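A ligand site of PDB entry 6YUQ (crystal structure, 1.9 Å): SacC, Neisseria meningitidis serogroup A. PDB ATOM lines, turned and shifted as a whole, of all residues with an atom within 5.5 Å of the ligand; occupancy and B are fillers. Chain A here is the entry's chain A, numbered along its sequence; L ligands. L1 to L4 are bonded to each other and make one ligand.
OD1 of Asn 230 sits at hydrogen-bond distance from O3 of LIG L1 (2.8 Å). N of Lys 43 sits at hydrogen-bond distance from O6 of LG3 L3, 3.4 Å away. The guanidinium group (NH2) of Arg 148 lies within salt-bridge range of an oxygen (O6) of LG3 L3 (3.0 Å). OG of Ser 114 is in hydrogen-bond range of O1 of LG2 L2. O3 of LG4 L4 sits at hydrogen-bond distance from O of Thr 147 (3.2 Å). The side-chain hydroxyl of Ser 113 sits at hydrogen-bond distance from an oxygen (O5) of LG2 L2. An oxygen (O2) of LG2 L2 sits close to the backbone carbonyl oxygen (O) of Phe 40 (3.3 Å). The guanidinium group (NH1) of Arg 76 lies within salt-bridge range of an oxygen (O6) of LG3 L3, 2.6 Å away.
OD2 of Asp 229 lies within hydrogen-bond range of N of Gly 227 (3.0 Å). The backbone carbonyl oxygen (O) of Pro 41 sits at hydrogen-bond distance from the guanidinium group (NH2) of Arg 148, at 3.3 Å. The side-chain amide oxygen (OD1) of Asn 50 sits close to the backbone carbonyl oxygen (O) of Lys 48 (3.3 Å). The backbone NH (N) of Ser 114 sits at hydrogen-bond distance from the backbone carbonyl oxygen (O) of Asn 135 (2.9 Å). O of Phe 40 sits at hydrogen-bond distance from NH2 of Arg 148. The backbone carbonyl oxygen (O) of Arg 76 is in hydrogen-bond range of the side-chain amino group (NZ) of Lys 115 (2.8 Å). The guanidinium group (NH1) of Arg 76 lies within hydrogen-bond range of the backbone carbonyl oxygen (O) of Pro 41 (3.0 Å). A ring nitrogen (NE2) of His 228 lies within hydrogen-bond range of the side-chain hydroxyl (OG) of Ser 114 (2.8 Å).
Residues that only touch the ligand: Ala 39 (3.7 Å), Pro 41 (3.6 Å), Pro 42 (3.5 Å), Asn 50 (3.9 Å), Lys 53 (3.6 Å), Tyr 144 (3.9 Å), Ser 149 (3.8 Å), His 228 (3.6 Å), Asp 229 (3.9 Å), Ile 233 (3.4 Å) and Arg 237 (3.7 Å). Hydrophobic or aromatic side chains within 4 Å of the ligand: Ala 39, Pro 42, His 228 and Ile 233. Within 4 Å of the ligand: Ala 39, Phe 40, Pro 41, Pro 42, Lys 43, Asn 50, Lys 53, Arg 76, Ser 113, Ser 114, Tyr 144, Thr 147, Arg 148, Ser 149, His 228, Asp 229, Asn 230, Ile 233 and Arg 237. The nearest printed residue that does not touch the ligand is Lys 146 (4.1 Å).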
ATOM      1  N   SER A  38     -13.369  -8.741  18.196  1.00  0.00           N
ATOM      2  CA  SER A  38     -12.206  -9.621  18.306  1.00  0.00           C
ATOM      3  C   SER A  38     -12.538 -11.013  17.787  1.00  0.00           C
ATOM      4  O   SER A  38     -13.667 -11.502  17.905  1.00  0.00           O
ATOM      5  CB  SER A  38     -11.753  -9.708  19.762  1.00  0.00           C
ATOM      6  OG  SER A  38     -10.779 -10.718  19.962  1.00  0.00           O
ATOM      7  N   ALA A  39     -11.528 -11.662  17.208  1.00  0.00           N
ATOM      8  CA  ALA A  39     -11.621 -13.047  16.757  1.00  0.00           C
ATOM      9  C   ALA A  39     -10.997 -13.993  17.785  1.00  0.00           C
ATOM     10  O   ALA A  39     -10.455 -13.563  18.808  1.00  0.00           O
ATOM     11  CB  ALA A  39     -10.949 -13.215  15.400  1.00  0.00           C
ATOM     12  N   PHE A  40     -11.093 -15.294  17.525  1.00  0.00           N
ATOM     13  CA  PHE A  40     -10.453 -16.312  18.374  1.00  0.00           C
ATOM     14  C   PHE A  40      -8.943 -16.181  18.268  1.00  0.00           C
ATOM     15  O   PHE A  40      -8.394 -16.381  17.176  1.00  0.00           O
ATOM     16  CB  PHE A  40     -10.851 -17.749  17.950  1.00  0.00           C
ATOM     17  CG  PHE A  40     -12.080 -18.274  18.649  1.00  0.00           C
ATOM     18  CD1 PHE A  40     -12.308 -18.002  19.986  1.00  0.00           C
ATOM     19  CD2 PHE A  40     -12.995 -19.059  17.963  1.00  0.00           C
ATOM     20  CE1 PHE A  40     -13.442 -18.486  20.634  1.00  0.00           C
ATOM     21  CE2 PHE A  40     -14.137 -19.547  18.601  1.00  0.00           C
ATOM     22  CZ  PHE A  40     -14.356 -19.258  19.942  1.00  0.00           C
ATOM     23  N   PRO A  41      -8.229 -15.841  19.332  1.00  0.00           N
ATOM     24  CA  PRO A  41      -6.766 -15.850  19.289  1.00  0.00           C
ATOM     25  C   PRO A  41      -6.258 -17.270  19.441  1.00  0.00           C
ATOM     26  O   PRO A  41      -7.034 -18.175  19.787  1.00  0.00           O
ATOM     27  CB  PRO A  41      -6.392 -14.991  20.499  1.00  0.00           C
ATOM     28  CG  PRO A  41      -7.467 -15.296  21.489  1.00  0.00           C
ATOM     29  CD  PRO A  41      -8.738 -15.464  20.664  1.00  0.00           C
ATOM     30  N   PRO A  42      -4.970 -17.525  19.166  1.00  0.00           N
ATOM     31  CA  PRO A  42      -4.414 -18.859  19.435  1.00  0.00           C
ATOM     32  C   PRO A  42      -4.502 -19.184  20.917  1.00  0.00           C
ATOM     33  O   PRO A  42      -4.612 -18.307  21.776  1.00  0.00           O
ATOM     34  CB  PRO A  42      -2.950 -18.748  18.975  1.00  0.00           C
ATOM     35  CG  PRO A  42      -2.946 -17.588  18.025  1.00  0.00           C
ATOM     36  CD  PRO A  42      -3.958 -16.623  18.592  1.00  0.00           C
ATOM     37  N   LYS A  43      -4.425 -20.479  21.222  1.00  0.00           N
ATOM     38  CA  LYS A  43      -4.567 -20.923  22.597  1.00  0.00           C
ATOM     39  C   LYS A  43      -3.470 -20.312  23.461  1.00  0.00           C
ATOM     40  O   LYS A  43      -2.325 -20.151  23.025  1.00  0.00           O
ATOM     41  CB  LYS A  43      -4.513 -22.455  22.685  1.00  0.00           C
ATOM     42  CG  LYS A  43      -4.560 -22.987  24.117  1.00  0.00           C
ATOM     43  CD  LYS A  43      -4.783 -24.491  24.172  1.00  0.00           C
ATOM     44  CE  LYS A  43      -4.388 -25.056  25.528  1.00  0.00           C
ATOM     45  NZ  LYS A  43      -5.368 -24.651  26.581  1.00  0.00           N
ATOM     46  N   LYS A  48      -7.534 -10.086  21.511  1.00  0.00           N
ATOM     47  CA  LYS A  48      -6.902  -8.894  20.963  1.00  0.00           C
ATOM     48  C   LYS A  48      -7.946  -7.950  20.362  1.00  0.00           C
ATOM     49  O   LYS A  48      -8.898  -8.400  19.715  1.00  0.00           O
ATOM     50  CB  LYS A  48      -5.859  -9.263  19.909  1.00  0.00           C
ATOM     51  N   TYR A  49      -7.761  -6.654  20.588  1.00  0.00           N
ATOM     52  CA  TYR A  49      -8.562  -5.658  19.905  1.00  0.00           C
ATOM     53  C   TYR A  49      -8.110  -5.538  18.458  1.00  0.00           C
ATOM     54  O   TYR A  49      -6.920  -5.642  18.160  1.00  0.00           O
ATOM     55  CB  TYR A  49      -8.457  -4.306  20.615  1.00  0.00           C
ATOM     56  CG  TYR A  49      -9.020  -4.320  22.009  1.00  0.00           C
ATOM     57  CD1 TYR A  49     -10.382  -4.198  22.230  1.00  0.00           C
ATOM     58  CD2 TYR A  49      -8.184  -4.450  23.121  1.00  0.00           C
ATOM     59  CE1 TYR A  49     -10.915  -4.212  23.501  1.00  0.00           C
ATOM     60  CE2 TYR A  49      -8.712  -4.447  24.409  1.00  0.00           C
ATOM     61  CZ  TYR A  49     -10.080  -4.336  24.591  1.00  0.00           C
ATOM     62  OH  TYR A  49     -10.628  -4.338  25.850  1.00  0.00           O
ATOM     63  N   ASN A  50      -9.051  -5.332  17.559  1.00  0.00           N
ATOM     64  CA  ASN A  50      -8.799  -5.444  16.132  1.00  0.00           C
ATOM     65  C   ASN A  50      -8.769  -4.074  15.458  1.00  0.00           C
ATOM     66  O   ASN A  50      -9.605  -3.206  15.742  1.00  0.00           O
ATOM     67  CB  ASN A  50      -9.857  -6.321  15.471  1.00  0.00           C
ATOM     68  CG  ASN A  50      -9.474  -7.782  15.444  1.00  0.00           C
ATOM     69  OD1 ASN A  50      -9.241  -8.407  16.483  1.00  0.00           O
ATOM     70  ND2 ASN A  50      -9.389  -8.337  14.257  1.00  0.00           N
ATOM     71  N   TYR A  51      -7.789  -3.903  14.570  1.00  0.00           N
ATOM     72  CA  TYR A  51      -7.702  -2.788  13.618  1.00  0.00           C
ATOM     73  C   TYR A  51      -7.500  -1.435  14.304  1.00  0.00           C
ATOM     74  O   TYR A  51      -7.903  -0.407  13.758  1.00  0.00           O
ATOM     75  CB  TYR A  51      -8.923  -2.752  12.699  1.00  0.00           C
ATOM     76  CG  TYR A  51      -9.324  -4.136  12.205  1.00  0.00           C
ATOM     77  CD1 TYR A  51      -8.375  -5.043  11.735  1.00  0.00           C
ATOM     78  CD2 TYR A  51     -10.646  -4.521  12.226  1.00  0.00           C
ATOM     79  CE1 TYR A  51      -8.739  -6.312  11.306  1.00  0.00           C
ATOM     80  CE2 TYR A  51     -11.037  -5.776  11.804  1.00  0.00           C
ATOM     81  CZ  TYR A  51     -10.088  -6.664  11.344  1.00  0.00           C
ATOM     82  OH  TYR A  51     -10.520  -7.912  10.933  1.00  0.00           O
ATOM     83  N   LYS A  53      -4.605   0.133  14.636  1.00  0.00           N
ATOM     84  CA  LYS A  53      -3.672   0.958  13.878  1.00  0.00           C
ATOM     85  C   LYS A  53      -4.285   1.528  12.608  1.00  0.00           C
ATOM     86  O   LYS A  53      -3.778   2.536  12.091  1.00  0.00           O
ATOM     87  CB  LYS A  53      -2.412   0.152  13.549  1.00  0.00           C
ATOM     88  CG  LYS A  53      -1.850  -0.645  14.719  1.00  0.00           C
ATOM     89  CD  LYS A  53      -0.520  -1.281  14.344  1.00  0.00           C
ATOM     90  CE  LYS A  53      -0.086  -2.322  15.369  1.00  0.00           C
ATOM     91  NZ  LYS A  53       0.936  -3.263  14.821  1.00  0.00           N
ATOM     92  N   ARG A  76     -11.074 -17.424  25.752  1.00  0.00           N
ATOM     93  CA  ARG A  76     -11.060 -16.787  24.438  1.00  0.00           C
ATOM     94  C   ARG A  76     -12.440 -16.415  23.936  1.00  0.00           C
ATOM     95  O   ARG A  76     -12.569 -15.983  22.786  1.00  0.00           O
ATOM     96  CB  ARG A  76     -10.353 -17.706  23.434  1.00  0.00           C
ATOM     97  CG  ARG A  76      -8.868 -17.803  23.715  1.00  0.00           C
ATOM     98  CD  ARG A  76      -8.161 -18.727  22.733  1.00  0.00           C
ATOM     99  NE  ARG A  76      -8.382 -20.148  23.024  1.00  0.00           N
ATOM    100  CZ  ARG A  76      -8.158 -21.114  22.137  1.00  0.00           C
ATOM    101  NH1 ARG A  76      -7.707 -20.830  20.932  1.00  0.00           N
ATOM    102  NH2 ARG A  76      -8.362 -22.384  22.483  1.00  0.00           N
ATOM    103  N   SER A 113     -13.285 -10.091  11.479  1.00  0.00           N
ATOM    104  CA  SER A 113     -12.944 -11.236  10.640  1.00  0.00           C
ATOM    105  C   SER A 113     -13.150 -12.517  11.434  1.00  0.00           C
ATOM    106  O   SER A 113     -12.899 -12.544  12.654  1.00  0.00           O
ATOM    107  CB  SER A 113     -11.493 -11.128  10.125  1.00  0.00           C
ATOM    108  OG  SER A 113     -11.126 -12.287   9.388  1.00  0.00           O
ATOM    109  N   SER A 114     -13.621 -13.567  10.764  1.00  0.00           N
ATOM    110  CA  SER A 114     -13.846 -14.890  11.386  1.00  0.00           C
ATOM    111  C   SER A 114     -14.846 -14.726  12.525  1.00  0.00           C
ATOM    112  O   SER A 114     -15.971 -14.269  12.258  1.00  0.00           O
ATOM    113  CB  SER A 114     -12.497 -15.486  11.779  1.00  0.00           C
ATOM    114  OG  SER A 114     -12.608 -16.884  12.015  1.00  0.00           O
ATOM    115  N   LYS A 115     -14.513 -15.103  13.761  1.00  0.00           N
ATOM    116  CA  LYS A 115     -15.451 -14.931  14.872  1.00  0.00           C
ATOM    117  C   LYS A 115     -15.826 -13.459  15.036  1.00  0.00           C
ATOM    118  O   LYS A 115     -16.957 -13.138  15.412  1.00  0.00           O
ATOM    119  CB  LYS A 115     -14.860 -15.471  16.168  1.00  0.00           C
ATOM    120  CG  LYS A 115     -15.822 -15.388  17.369  1.00  0.00           C
ATOM    121  CD  LYS A 115     -15.138 -15.751  18.683  1.00  0.00           C
ATOM    122  CE  LYS A 115     -14.269 -14.612  19.202  1.00  0.00           C
ATOM    123  NZ  LYS A 115     -13.781 -14.852  20.589  1.00  0.00           N
ATOM    124  N   ASN A 135     -14.951 -10.190   7.119  1.00  0.00           N
ATOM    125  CA  ASN A 135     -14.211 -11.183   6.355  1.00  0.00           C
ATOM    126  C   ASN A 135     -14.448 -12.572   6.939  1.00  0.00           C
ATOM    127  O   ASN A 135     -14.487 -12.734   8.161  1.00  0.00           O
ATOM    128  CB  ASN A 135     -12.714 -10.882   6.340  1.00  0.00           C
ATOM    129  CG  ASN A 135     -11.919 -11.944   5.600  1.00  0.00           C
ATOM    130  OD1 ASN A 135     -11.989 -12.037   4.378  1.00  0.00           O
ATOM    131  ND2 ASN A 135     -11.184 -12.757   6.346  1.00  0.00           N
ATOM    132  N   TYR A 144     -17.528 -24.949  14.020  1.00  0.00           N
ATOM    133  CA  TYR A 144     -16.247 -24.271  13.983  1.00  0.00           C
ATOM    134  C   TYR A 144     -15.580 -24.231  15.348  1.00  0.00           C
ATOM    135  O   TYR A 144     -14.360 -24.398  15.444  1.00  0.00           O
ATOM    136  CB  TYR A 144     -16.396 -22.857  13.431  1.00  0.00           C
ATOM    137  CG  TYR A 144     -15.057 -22.143  13.310  1.00  0.00           C
ATOM    138  CD1 TYR A 144     -14.166 -22.474  12.289  1.00  0.00           C
ATOM    139  CD2 TYR A 144     -14.682 -21.153  14.206  1.00  0.00           C
ATOM    140  CE1 TYR A 144     -12.939 -21.838  12.159  1.00  0.00           C
ATOM    141  CE2 TYR A 144     -13.454 -20.510  14.092  1.00  0.00           C
ATOM    142  CZ  TYR A 144     -12.584 -20.850  13.064  1.00  0.00           C
ATOM    143  OH  TYR A 144     -11.370 -20.221  12.938  1.00  0.00           O
ATOM    144  N   LYS A 146     -15.806 -26.414  17.558  1.00  0.00           N
ATOM    145  CA  LYS A 146     -15.277 -27.759  17.737  1.00  0.00           C
ATOM    146  C   LYS A 146     -13.868 -27.876  17.191  1.00  0.00           C
ATOM    147  O   LYS A 146     -13.019 -28.561  17.773  1.00  0.00           O
ATOM    148  CB  LYS A 146     -16.200 -28.771  17.052  1.00  0.00           C
ATOM    149  CG  LYS A 146     -15.986 -30.200  17.466  1.00  0.00           C
ATOM    150  CD  LYS A 146     -17.142 -31.074  17.014  1.00  0.00           C
ATOM    151  CE  LYS A 146     -17.107 -31.309  15.522  1.00  0.00           C
ATOM    152  NZ  LYS A 146     -17.524 -32.705  15.214  1.00  0.00           N
ATOM    153  N   THR A 147     -13.589 -27.208  16.079  1.00  0.00           N
ATOM    154  CA  THR A 147     -12.265 -27.272  15.454  1.00  0.00           C
ATOM    155  C   THR A 147     -11.257 -26.325  16.077  1.00  0.00           C
ATOM    156  O   THR A 147     -10.100 -26.311  15.647  1.00  0.00           O
ATOM    157  CB  THR A 147     -12.359 -26.962  13.956  1.00  0.00           C
ATOM    158  OG1 THR A 147     -12.418 -25.545  13.777  1.00  0.00           O
ATOM    159  CG2 THR A 147     -13.599 -27.602  13.345  1.00  0.00           C
ATOM    160  N   ARG A 148     -11.647 -25.527  17.072  1.00  0.00           N
ATOM    161  CA  ARG A 148     -10.764 -24.531  17.671  1.00  0.00           C
ATOM    162  C   ARG A 148     -10.475 -24.777  19.141  1.00  0.00           C
ATOM    163  O   ARG A 148      -9.347 -24.548  19.590  1.00  0.00           O
ATOM    164  CB  ARG A 148     -11.358 -23.120  17.508  1.00  0.00           C
ATOM    165  CG  ARG A 148     -11.260 -22.564  16.100  1.00  0.00           C
ATOM    166  CD  ARG A 148      -9.811 -22.571  15.589  1.00  0.00           C
ATOM    167  NE  ARG A 148      -8.943 -21.724  16.415  1.00  0.00           N
ATOM    168  CZ  ARG A 148      -8.895 -20.401  16.295  1.00  0.00           C
ATOM    169  NH1 ARG A 148      -9.658 -19.793  15.399  1.00  0.00           N
ATOM    170  NH2 ARG A 148      -8.093 -19.695  17.082  1.00  0.00           N
ATOM    171  N   SER A 149     -11.464 -25.231  19.928  1.00  0.00           N
ATOM    172  CA  SER A 149     -11.243 -25.498  21.348  1.00  0.00           C
ATOM    173  C   SER A 149     -12.378 -26.385  21.844  1.00  0.00           C
ATOM    174  O   SER A 149     -13.534 -25.939  21.892  1.00  0.00           O
ATOM    175  CB  SER A 149     -11.184 -24.200  22.151  1.00  0.00           C
ATOM    176  OG  SER A 149     -11.527 -24.427  23.502  1.00  0.00           O
ATOM    177  N   LYS A 150     -12.038 -27.609  22.237  1.00  0.00           N
ATOM    178  CA  LYS A 150     -13.038 -28.472  22.863  1.00  0.00           C
ATOM    179  C   LYS A 150     -13.472 -27.931  24.215  1.00  0.00           C
ATOM    180  O   LYS A 150     -14.620 -28.133  24.632  1.00  0.00           O
ATOM    181  CB  LYS A 150     -12.495 -29.895  22.995  1.00  0.00           C
ATOM    182  CG  LYS A 150     -12.220 -30.573  21.653  1.00  0.00           C
ATOM    183  CD  LYS A 150     -13.506 -30.965  20.931  1.00  0.00           C
ATOM    184  CE  LYS A 150     -13.254 -31.901  19.752  1.00  0.00           C
ATOM    185  NZ  LYS A 150     -12.514 -31.247  18.638  1.00  0.00           N
ATOM    186  N   GLY A 227      -5.800 -17.409   2.327  1.00  0.00           N
ATOM    187  CA  GLY A 227      -6.697 -18.344   2.976  1.00  0.00           C
ATOM    188  C   GLY A 227      -7.346 -17.713   4.186  1.00  0.00           C
ATOM    189  O   GLY A 227      -7.743 -16.536   4.127  1.00  0.00           O
ATOM    190  N   HIS A 228      -7.475 -18.478   5.273  1.00  0.00           N
ATOM    191  CA  HIS A 228      -7.904 -17.963   6.573  1.00  0.00           C
ATOM    192  C   HIS A 228      -6.668 -17.565   7.384  1.00  0.00           C
ATOM    193  O   HIS A 228      -6.343 -18.153   8.408  1.00  0.00           O
ATOM    194  CB  HIS A 228      -8.732 -19.014   7.312  1.00  0.00           C
ATOM    195  CG  HIS A 228      -9.726 -18.467   8.285  1.00  0.00           C
ATOM    196  ND1 HIS A 228     -10.973 -18.021   7.902  1.00  0.00           N
ATOM    197  CD2 HIS A 228      -9.658 -18.298   9.631  1.00  0.00           C
ATOM    198  CE1 HIS A 228     -11.629 -17.598   8.975  1.00  0.00           C
ATOM    199  NE2 HIS A 228     -10.858 -17.760  10.028  1.00  0.00           N
ATOM    200  N   ASP A 229      -6.002 -16.513   6.909  1.00  0.00           N
ATOM    201  CA  ASP A 229      -4.663 -16.177   7.405  1.00  0.00           C
ATOM    202  C   ASP A 229      -4.475 -14.657   7.363  1.00  0.00           C
ATOM    203  O   ASP A 229      -5.404 -13.905   7.073  1.00  0.00           O
ATOM    204  CB  ASP A 229      -3.593 -16.887   6.558  1.00  0.00           C
ATOM    205  CG  ASP A 229      -3.802 -16.656   5.066  1.00  0.00           C
ATOM    206  OD1 ASP A 229      -4.201 -15.541   4.684  1.00  0.00           O
ATOM    207  OD2 ASP A 229      -3.578 -17.598   4.277  1.00  0.00           O
ATOM    208  N   ASN A 230      -3.238 -14.221   7.618  1.00  0.00           N
ATOM    209  CA  ASN A 230      -2.920 -12.802   7.656  1.00  0.00           C
ATOM    210  C   ASN A 230      -2.925 -12.139   6.279  1.00  0.00           C
ATOM    211  O   ASN A 230      -3.107 -10.921   6.196  1.00  0.00           O
ATOM    212  CB  ASN A 230      -1.544 -12.606   8.321  1.00  0.00           C
ATOM    213  CG  ASN A 230      -1.639 -12.588   9.844  1.00  0.00           C
ATOM    214  OD1 ASN A 230      -2.647 -12.997  10.431  1.00  0.00           O
ATOM    215  ND2 ASN A 230      -0.582 -12.090  10.488  1.00  0.00           N
ATOM    216  N   ILE A 233      -6.483 -11.121   5.722  1.00  0.00           N
ATOM    217  CA  ILE A 233      -6.755  -9.992   6.616  1.00  0.00           C
ATOM    218  C   ILE A 233      -6.167  -8.713   6.048  1.00  0.00           C
ATOM    219  O   ILE A 233      -6.797  -7.646   6.098  1.00  0.00           O
ATOM    220  CB  ILE A 233      -6.233 -10.291   8.030  1.00  0.00           C
ATOM    221  CG1 ILE A 233      -7.186 -11.241   8.772  1.00  0.00           C
ATOM    222  CG2 ILE A 233      -6.089  -9.005   8.834  1.00  0.00           C
ATOM    223  CD1 ILE A 233      -6.580 -11.854   9.999  1.00  0.00           C
ATOM    224  N   ARG A 237      -8.385  -5.510   5.213  1.00  0.00           N
ATOM    225  CA  ARG A 237      -8.117  -4.161   5.718  1.00  0.00           C
ATOM    226  C   ARG A 237      -8.133  -3.134   4.589  1.00  0.00           C
ATOM    227  O   ARG A 237      -8.698  -2.052   4.725  1.00  0.00           O
ATOM    228  CB  ARG A 237      -6.761  -4.132   6.444  1.00  0.00           C
ATOM    229  CG  ARG A 237      -6.774  -4.640   7.895  1.00  0.00           C
ATOM    230  CD  ARG A 237      -5.388  -4.606   8.535  1.00  0.00           C
ATOM    231  NE  ARG A 237      -5.134  -3.420   9.369  1.00  0.00           N
ATOM    232  CZ  ARG A 237      -4.500  -3.456  10.541  1.00  0.00           C
ATOM    233  NH1 ARG A 237      -4.312  -2.352  11.232  1.00  0.00           N
ATOM    234  NH2 ARG A 237      -4.093  -4.613  11.033  1.00  0.00           N
HETATM  235  C1  LIG L   1      -3.475  -8.287  14.856  1.00  0.00           C
HETATM  236  C2  LIG L   1      -2.583  -8.302  13.626  1.00  0.00           C
HETATM  237  C3  LIG L   1      -2.730  -9.564  12.823  1.00  0.00           C
HETATM  238  C4  LIG L   1      -3.854 -10.453  13.300  1.00  0.00           C
HETATM  239  C5  LIG L   1      -5.132  -9.668  13.615  1.00  0.00           C
HETATM  240  C6  LIG L   1      -6.131 -10.564  14.333  1.00  0.00           C
HETATM  241  C7  LIG L   1      -0.427  -6.880  13.699  1.00  0.00           C
HETATM  242  C8  LIG L   1      -1.143  -5.768  12.873  1.00  0.00           C
HETATM  243  N1  LIG L   1      -1.152  -8.117  14.062  1.00  0.00           N
HETATM  244  O1  LIG L   1      -3.299  -7.106  15.542  1.00  0.00           O
HETATM  245  O2  LIG L   1      -1.483 -10.308  12.850  1.00  0.00           O
HETATM  246  O3  LIG L   1      -4.125 -11.451  12.300  1.00  0.00           O
HETATM  247  O4  LIG L   1      -4.910  -8.465  14.449  1.00  0.00           O
HETATM  248  O5  LIG L   1      -5.446 -11.732  14.829  1.00  0.00           O
HETATM  249  O6  LIG L   1       0.689  -6.725  14.044  1.00  0.00           O
HETATM  250  P1  LIG L   1      -6.254 -12.769  15.907  1.00  0.00           P
HETATM  251  O7  LIG L   1      -7.015 -11.951  16.924  1.00  0.00           O
HETATM  252  O8  LIG L   1      -5.244 -13.633  16.639  1.00  0.00           O
HETATM  253  O9  LIG L   1      -7.317 -13.714  15.056  1.00  0.00           O
HETATM  254  C1  LG2 L   2      -7.019 -14.084  13.782  1.00  0.00           C
HETATM  255  C2  LG2 L   2      -8.211 -14.840  13.211  1.00  0.00           C
HETATM  256  C3  LG2 L   2      -8.426 -16.144  13.876  1.00  0.00           C
HETATM  257  C4  LG2 L   2      -7.155 -16.967  13.888  1.00  0.00           C
HETATM  258  C5  LG2 L   2      -6.019 -16.169  14.557  1.00  0.00           C
HETATM  259  C6  LG2 L   2      -4.750 -16.970  14.629  1.00  0.00           C
HETATM  260  C7  LG2 L   2      -8.804 -14.498  10.741  1.00  0.00           C
HETATM  261  C8  LG2 L   2      -8.565 -14.823   9.263  1.00  0.00           C
HETATM  262  N1  LG2 L   2      -7.983 -15.143  11.762  1.00  0.00           N
HETATM  263  O1  LG2 L   2      -9.484 -16.850  13.178  1.00  0.00           O
HETATM  264  O2  LG2 L   2      -7.364 -18.177  14.584  1.00  0.00           O
HETATM  265  O3  LG2 L   2      -5.769 -14.922  13.809  1.00  0.00           O
HETATM  266  O4  LG2 L   2      -4.515 -17.568  13.334  1.00  0.00           O
HETATM  267  O5  LG2 L   2      -9.660 -13.721  11.064  1.00  0.00           O
HETATM  268  P1  LG2 L   2      -2.935 -17.713  12.812  1.00  0.00           P
HETATM  269  O6  LG2 L   2      -2.064 -16.709  13.555  1.00  0.00           O
HETATM  270  O7  LG2 L   2      -2.858 -17.483  11.312  1.00  0.00           O
HETATM  271  O8  LG2 L   2      -2.398 -19.268  13.174  1.00  0.00           O
HETATM  272  C1  LG3 L   3      -2.043 -19.523  14.485  1.00  0.00           C
HETATM  273  C2  LG3 L   3      -1.116 -20.714  14.532  1.00  0.00           C
HETATM  274  C3  LG3 L   3      -1.769 -21.918  13.996  1.00  0.00           C
HETATM  275  C4  LG3 L   3      -3.079 -22.201  14.685  1.00  0.00           C
HETATM  276  C5  LG3 L   3      -3.998 -20.981  14.746  1.00  0.00           C
HETATM  277  C6  LG3 L   3      -5.152 -21.301  15.682  1.00  0.00           C
HETATM  278  C7  LG3 L   3       0.596 -20.642  16.484  1.00  0.00           C
HETATM  279  C8  LG3 L   3       1.671 -20.080  15.538  1.00  0.00           C
HETATM  280  N1  LG3 L   3      -0.745 -20.954  15.989  1.00  0.00           N
HETATM  281  O1  LG3 L   3      -0.882 -23.066  14.145  1.00  0.00           O
HETATM  282  O2  LG3 L   3      -3.744 -23.266  13.980  1.00  0.00           O
HETATM  283  O3  LG3 L   3      -3.305 -19.779  15.249  1.00  0.00           O
HETATM  284  O4  LG3 L   3      -4.576 -21.595  16.950  1.00  0.00           O
HETATM  285  O5  LG3 L   3       0.848 -20.838  17.630  1.00  0.00           O
HETATM  286  P1  LG3 L   3      -5.474 -22.495  18.043  1.00  0.00           P
HETATM  287  O6  LG3 L   3      -6.445 -21.581  18.736  1.00  0.00           O
HETATM  288  O7  LG3 L   3      -4.653 -23.163  19.113  1.00  0.00           O
HETATM  289  O8  LG3 L   3      -6.437 -23.555  17.158  1.00  0.00           O
HETATM  290  C1  LG4 L   4      -6.071 -24.845  16.883  1.00  0.00           C
HETATM  291  C2  LG4 L   4      -6.766 -25.258  15.589  1.00  0.00           C
HETATM  292  N1  LG4 L   4      -6.426 -24.354  14.419  1.00  0.00           N
HETATM  293  C3  LG4 L   4      -7.377 -24.240  13.296  1.00  0.00           C
HETATM  294  O1  LG4 L   4      -8.390 -24.871  13.310  1.00  0.00           O
HETATM  295  C4  LG4 L   4      -7.052 -23.294  12.080  1.00  0.00           C
HETATM  296  C5  LG4 L   4      -6.444 -26.679  15.283  1.00  0.00           C
HETATM  297  O2  LG4 L   4      -5.009 -26.818  15.066  1.00  0.00           O
HETATM  298  C6  LG4 L   4      -6.837 -27.571  16.424  1.00  0.00           C
HETATM  299  O3  LG4 L   4      -7.813 -28.491  15.909  1.00  0.00           O
HETATM  300  C7  LG4 L   4      -7.428 -26.767  17.606  1.00  0.00           C
HETATM  301  C8  LG4 L   4      -7.730 -27.665  18.810  1.00  0.00           C
HETATM  302  O4  LG4 L   4      -9.107 -27.991  18.754  1.00  0.00           O
HETATM  303  O5  LG4 L   4      -6.527 -25.695  18.040  1.00  0.00           O
